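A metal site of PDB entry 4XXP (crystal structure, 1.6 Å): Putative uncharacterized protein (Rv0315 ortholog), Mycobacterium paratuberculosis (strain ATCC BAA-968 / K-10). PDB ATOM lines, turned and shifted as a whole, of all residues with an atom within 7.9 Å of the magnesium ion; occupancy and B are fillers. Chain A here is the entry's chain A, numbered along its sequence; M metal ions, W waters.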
ATOM      1  N   ASP A  29      -0.083 -27.324 -20.826  1.00  0.00           N
ATOM      2  CA  ASP A  29      -0.157 -26.127 -21.648  1.00  0.00           C
ATOM      3  C   ASP A  29      -1.618 -25.736 -21.790  1.00  0.00           C
ATOM      4  O   ASP A  29      -2.446 -26.554 -22.181  1.00  0.00           O
ATOM      5  CB  ASP A  29       0.485 -26.343 -23.022  1.00  0.00           C
ATOM      6  CG  ASP A  29       0.877 -25.039 -23.703  1.00  0.00           C
ATOM      7  OD1 ASP A  29       0.326 -23.958 -23.352  1.00  0.00           O
ATOM      8  OD2 ASP A  29       1.745 -25.097 -24.581  1.00  0.00           O
ATOM      9  N   GLU A  30      -1.927 -24.484 -21.473  1.00  0.00           N
ATOM     10  CA  GLU A  30      -3.290 -23.958 -21.602  1.00  0.00           C
ATOM     11  C   GLU A  30      -3.479 -23.269 -22.947  1.00  0.00           C
ATOM     12  O   GLU A  30      -4.582 -22.824 -23.280  1.00  0.00           O
ATOM     13  CB  GLU A  30      -3.566 -22.998 -20.448  1.00  0.00           C
ATOM     14  CG  GLU A  30      -3.369 -23.647 -19.083  1.00  0.00           C
ATOM     15  CD  GLU A  30      -4.372 -24.752 -18.801  1.00  0.00           C
ATOM     16  OE1 GLU A  30      -5.523 -24.692 -19.294  1.00  0.00           O
ATOM     17  OE2 GLU A  30      -4.004 -25.699 -18.073  1.00  0.00           O
ATOM     18  N   PHE A  31      -2.388 -23.184 -23.711  1.00  0.00           N
ATOM     19  CA  PHE A  31      -2.394 -22.588 -25.050  1.00  0.00           C
ATOM     20  C   PHE A  31      -2.981 -21.163 -25.058  1.00  0.00           C
ATOM     21  O   PHE A  31      -3.661 -20.732 -25.996  1.00  0.00           O
ATOM     22  CB  PHE A  31      -3.151 -23.505 -26.033  1.00  0.00           C
ATOM     23  CG  PHE A  31      -2.501 -24.856 -26.181  1.00  0.00           C
ATOM     24  CD1 PHE A  31      -1.197 -24.957 -26.677  1.00  0.00           C
ATOM     25  CD2 PHE A  31      -3.152 -26.004 -25.773  1.00  0.00           C
ATOM     26  CE1 PHE A  31      -0.574 -26.188 -26.806  1.00  0.00           C
ATOM     27  CE2 PHE A  31      -2.536 -27.240 -25.899  1.00  0.00           C
ATOM     28  CZ  PHE A  31      -1.236 -27.331 -26.416  1.00  0.00           C
ATOM     29  N   ASP A  32      -2.664 -20.413 -24.004  1.00  0.00           N
ATOM     30  CA  ASP A  32      -3.002 -18.994 -23.958  1.00  0.00           C
ATOM     31  C   ASP A  32      -1.948 -18.214 -24.733  1.00  0.00           C
ATOM     32  O   ASP A  32      -0.760 -18.546 -24.712  1.00  0.00           O
ATOM     33  CB  ASP A  32      -3.079 -18.484 -22.507  1.00  0.00           C
ATOM     34  CG  ASP A  32      -4.232 -19.078 -21.704  1.00  0.00           C
ATOM     35  OD1 ASP A  32      -5.324 -19.305 -22.262  1.00  0.00           O
ATOM     36  OD2 ASP A  32      -4.032 -19.297 -20.484  1.00  0.00           O
ATOM     37  N   GLY A  33      -2.384 -17.160 -25.408  1.00  0.00           N
ATOM     38  CA  GLY A  33      -1.443 -16.351 -26.173  1.00  0.00           C
ATOM     39  C   GLY A  33      -2.115 -15.674 -27.327  1.00  0.00           C
ATOM     40  O   GLY A  33      -3.238 -16.035 -27.680  1.00  0.00           O
ATOM     41  N   ASP A  78      -5.147 -19.549 -31.296  1.00  0.00           N
ATOM     42  CA  ASP A  78      -6.218 -18.734 -31.879  1.00  0.00           C
ATOM     43  C   ASP A  78      -6.566 -17.482 -31.068  1.00  0.00           C
ATOM     44  O   ASP A  78      -7.426 -16.718 -31.487  1.00  0.00           O
ATOM     45  CB  ASP A  78      -7.485 -19.592 -32.105  1.00  0.00           C
ATOM     46  CG  ASP A  78      -8.167 -20.083 -30.803  1.00  0.00           C
ATOM     47  OD1 ASP A  78      -7.643 -19.840 -29.687  1.00  0.00           O
ATOM     48  OD2 ASP A  78      -9.220 -20.745 -30.919  1.00  0.00           O
ATOM     49  N   LYS A  80      -7.892 -17.458 -28.180  1.00  0.00           N
ATOM     50  CA  LYS A  80      -9.032 -17.790 -27.327  1.00  0.00           C
ATOM     51  C   LYS A  80      -8.722 -18.998 -26.461  1.00  0.00           C
ATOM     52  O   LYS A  80      -9.637 -19.711 -25.999  1.00  0.00           O
ATOM     53  CB  LYS A  80     -10.277 -18.065 -28.197  1.00  0.00           C
ATOM     54  CG  LYS A  80     -10.621 -16.943 -29.149  1.00  0.00           C
ATOM     55  CD  LYS A  80     -11.820 -17.294 -30.047  1.00  0.00           C
ATOM     56  CE  LYS A  80     -12.011 -16.228 -31.127  1.00  0.00           C
ATOM     57  NZ  LYS A  80     -13.289 -16.356 -31.897  1.00  0.00           N
ATOM     58  N   SER A  81      -7.424 -19.248 -26.271  1.00  0.00           N
ATOM     59  CA  SER A  81      -6.878 -20.312 -25.404  1.00  0.00           C
ATOM     60  C   SER A  81      -6.806 -21.687 -26.106  1.00  0.00           C
ATOM     61  O   SER A  81      -6.653 -22.712 -25.440  1.00  0.00           O
ATOM     62  CB  SER A  81      -7.681 -20.423 -24.086  1.00  0.00           C
ATOM     63  OG  SER A  81      -7.027 -21.234 -23.133  1.00  0.00           O
ATOM     64  N   ASN A  82      -6.881 -21.712 -27.434  1.00  0.00           N
ATOM     65  CA  ASN A  82      -6.745 -22.961 -28.155  1.00  0.00           C
ATOM     66  C   ASN A  82      -5.553 -22.997 -29.087  1.00  0.00           C
ATOM     67  O   ASN A  82      -5.243 -22.009 -29.766  1.00  0.00           O
ATOM     68  CB  ASN A  82      -8.001 -23.233 -28.990  1.00  0.00           C
ATOM     69  CG  ASN A  82      -9.264 -23.066 -28.188  1.00  0.00           C
ATOM     70  OD1 ASN A  82      -9.405 -23.668 -27.117  1.00  0.00           O
ATOM     71  ND2 ASN A  82     -10.168 -22.223 -28.657  1.00  0.00           N
ATOM     72  N   LEU A  83      -4.903 -24.159 -29.142  1.00  0.00           N
ATOM     73  CA  LEU A  83      -4.007 -24.502 -30.241  1.00  0.00           C
ATOM     74  C   LEU A  83      -4.882 -25.005 -31.386  1.00  0.00           C
ATOM     75  O   LEU A  83      -5.768 -25.840 -31.145  1.00  0.00           O
ATOM     76  CB  LEU A  83      -3.008 -25.588 -29.806  1.00  0.00           C
ATOM     77  CG  LEU A  83      -2.225 -26.240 -30.937  1.00  0.00           C
ATOM     78  CD1 LEU A  83      -1.308 -25.187 -31.613  1.00  0.00           C
ATOM     79  CD2 LEU A  83      -1.428 -27.412 -30.394  1.00  0.00           C
ATOM     80  N   ARG A 114      -8.334 -31.373 -23.592  1.00  0.00           N
ATOM     81  CA  ARG A 114      -9.650 -30.905 -24.043  1.00  0.00           C
ATOM     82  C   ARG A 114      -9.551 -30.581 -25.520  1.00  0.00           C
ATOM     83  O   ARG A 114      -8.730 -29.735 -25.926  1.00  0.00           O
ATOM     84  CB  ARG A 114     -10.085 -29.680 -23.241  1.00  0.00           C
ATOM     85  CG  ARG A 114     -11.508 -29.232 -23.592  1.00  0.00           C
ATOM     86  CD  ARG A 114     -12.013 -28.202 -22.616  1.00  0.00           C
ATOM     87  NE  ARG A 114     -13.439 -27.932 -22.789  1.00  0.00           N
ATOM     88  CZ  ARG A 114     -13.928 -26.828 -23.342  1.00  0.00           C
ATOM     89  NH1 ARG A 114     -13.109 -25.879 -23.815  1.00  0.00           N
ATOM     90  NH2 ARG A 114     -15.247 -26.677 -23.431  1.00  0.00           N
ATOM     91  N   TRP A 175     -16.771 -29.872 -28.001  1.00  0.00           N
ATOM     92  CA  TRP A 175     -15.702 -30.010 -27.020  1.00  0.00           C
ATOM     93  C   TRP A 175     -15.867 -31.268 -26.175  1.00  0.00           C
ATOM     94  O   TRP A 175     -16.966 -31.536 -25.661  1.00  0.00           O
ATOM     95  CB  TRP A 175     -15.634 -28.803 -26.080  1.00  0.00           C
ATOM     96  CG  TRP A 175     -15.037 -27.581 -26.687  1.00  0.00           C
ATOM     97  CD1 TRP A 175     -15.701 -26.421 -27.049  1.00  0.00           C
ATOM     98  CD2 TRP A 175     -13.668 -27.374 -27.001  1.00  0.00           C
ATOM     99  NE1 TRP A 175     -14.811 -25.510 -27.553  1.00  0.00           N
ATOM    100  CE2 TRP A 175     -13.562 -26.070 -27.567  1.00  0.00           C
ATOM    101  CE3 TRP A 175     -12.528 -28.156 -26.885  1.00  0.00           C
ATOM    102  CZ2 TRP A 175     -12.334 -25.534 -27.980  1.00  0.00           C
ATOM    103  CZ3 TRP A 175     -11.292 -27.627 -27.317  1.00  0.00           C
ATOM    104  CH2 TRP A 175     -11.218 -26.330 -27.854  1.00  0.00           C
ATOM    105  N   ILE A 247      -7.243 -27.652 -29.636  1.00  0.00           N
ATOM    106  CA  ILE A 247      -6.906 -28.178 -28.323  1.00  0.00           C
ATOM    107  C   ILE A 247      -6.869 -27.052 -27.309  1.00  0.00           C
ATOM    108  O   ILE A 247      -6.066 -26.136 -27.453  1.00  0.00           O
ATOM    109  CB  ILE A 247      -5.566 -28.904 -28.331  1.00  0.00           C
ATOM    110  CG1 ILE A 247      -5.550 -29.997 -29.407  1.00  0.00           C
ATOM    111  CG2 ILE A 247      -5.298 -29.543 -26.959  1.00  0.00           C
ATOM    112  CD1 ILE A 247      -4.896 -29.555 -30.697  1.00  0.00           C
ATOM    113  N   ASP A 248      -7.740 -27.087 -26.307  1.00  0.00           N
ATOM    114  CA  ASP A 248      -7.813 -26.020 -25.315  1.00  0.00           C
ATOM    115  C   ASP A 248      -6.680 -26.175 -24.292  1.00  0.00           C
ATOM    116  O   ASP A 248      -6.103 -25.195 -23.824  1.00  0.00           O
ATOM    117  CB  ASP A 248      -9.199 -26.031 -24.646  1.00  0.00           C
ATOM    118  CG  ASP A 248      -9.456 -24.815 -23.728  1.00  0.00           C
ATOM    119  OD1 ASP A 248      -8.648 -23.856 -23.652  1.00  0.00           O
ATOM    120  OD2 ASP A 248     -10.543 -24.818 -23.103  1.00  0.00           O
ATOM    121  N   TRP A 249      -6.351 -27.404 -23.942  1.00  0.00           N
ATOM    122  CA  TRP A 249      -5.320 -27.620 -22.953  1.00  0.00           C
ATOM    123  C   TRP A 249      -4.934 -29.069 -22.897  1.00  0.00           C
ATOM    124  O   TRP A 249      -5.691 -29.948 -23.326  1.00  0.00           O
ATOM    125  CB  TRP A 249      -5.747 -27.134 -21.538  1.00  0.00           C
ATOM    126  CG  TRP A 249      -7.138 -27.494 -21.054  1.00  0.00           C
ATOM    127  CD1 TRP A 249      -8.236 -26.660 -21.056  1.00  0.00           C
ATOM    128  CD2 TRP A 249      -7.576 -28.728 -20.469  1.00  0.00           C
ATOM    129  NE1 TRP A 249      -9.313 -27.300 -20.494  1.00  0.00           N
ATOM    130  CE2 TRP A 249      -8.940 -28.574 -20.131  1.00  0.00           C
ATOM    131  CE3 TRP A 249      -6.939 -29.951 -20.172  1.00  0.00           C
ATOM    132  CZ2 TRP A 249      -9.694 -29.589 -19.540  1.00  0.00           C
ATOM    133  CZ3 TRP A 249      -7.706 -30.964 -19.583  1.00  0.00           C
ATOM    134  CH2 TRP A 249      -9.056 -30.772 -19.275  1.00  0.00           C
ATOM    135  N   ILE A 250      -3.714 -29.318 -22.420  1.00  0.00           N
ATOM    136  CA  ILE A 250      -3.300 -30.639 -21.968  1.00  0.00           C
ATOM    137  C   ILE A 250      -2.719 -30.473 -20.562  1.00  0.00           C
ATOM    138  O   ILE A 250      -2.005 -29.509 -20.291  1.00  0.00           O
ATOM    139  CB  ILE A 250      -2.290 -31.274 -22.949  1.00  0.00           C
ATOM    140  CG1 ILE A 250      -1.888 -32.662 -22.446  1.00  0.00           C
ATOM    141  CG2 ILE A 250      -1.071 -30.351 -23.156  1.00  0.00           C
ATOM    142  CD1 ILE A 250      -1.123 -33.488 -23.455  1.00  0.00           C
ATOM    143  N   ARG A 251      -3.043 -31.417 -19.677  1.00  0.00           N
ATOM    144  CA  ARG A 251      -2.580 -31.372 -18.283  1.00  0.00           C
ATOM    145  C   ARG A 251      -2.178 -32.775 -17.857  1.00  0.00           C
ATOM    146  O   ARG A 251      -2.847 -33.747 -18.209  1.00  0.00           O
ATOM    147  CB  ARG A 251      -3.680 -30.858 -17.364  1.00  0.00           C
ATOM    148  CG  ARG A 251      -4.105 -29.419 -17.642  1.00  0.00           C
ATOM    149  CD  ARG A 251      -5.429 -29.099 -16.974  1.00  0.00           C
ATOM    150  NE  ARG A 251      -5.863 -27.780 -17.387  1.00  0.00           N
ATOM    151  CZ  ARG A 251      -7.132 -27.356 -17.319  1.00  0.00           C
ATOM    152  NH1 ARG A 251      -8.064 -28.163 -16.797  1.00  0.00           N
ATOM    153  NH2 ARG A 251      -7.454 -26.147 -17.742  1.00  0.00           N
HETATM  154 MG    MG M   1      -6.642 -23.223 -23.380  1.00  0.00          MG
HETATM  155  O   HOH W   1      -6.883 -23.471 -21.334  1.00  0.00           O
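OD1 of Asp 32 sits close to OG of Ser 81, at 2.7 Å. The side-chain carboxylate of Asp 78 lies within hydrogen-bond range of the backbone NH of Ser 81 (3.5 Å). The guanidinium group of Arg 114 lies within salt-bridge range of the side-chain carboxylate of Asp 248. The side-chain carboxylate (OE1) of Glu 30 is in salt-bridge range of the guanidinium group (NH2) of Arg 251 (2.9 Å).
Three residues have an atom within 4 Å of the magnesium ion: Glu 30, Ser 81 and Asp 248. The nearest printed residue that does not touch the magnesium ion is Trp 249 (4.2 Å).
The magnesium ion is bound by the side-chain hydroxyl (OG) of Ser 81 (2.0 Å), water W1 (2.1 Å), the backbone carbonyl oxygen (O) of Asp 248 (2.1 Å), the backbone carbonyl oxygen (O) of Glu 30 (2.1 Å), the side-chain carboxylate (OD1) of Asp 248 (2.1 Å) and the backbone carbonyl oxygen (O) of Ser 81 (2.1 Å).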
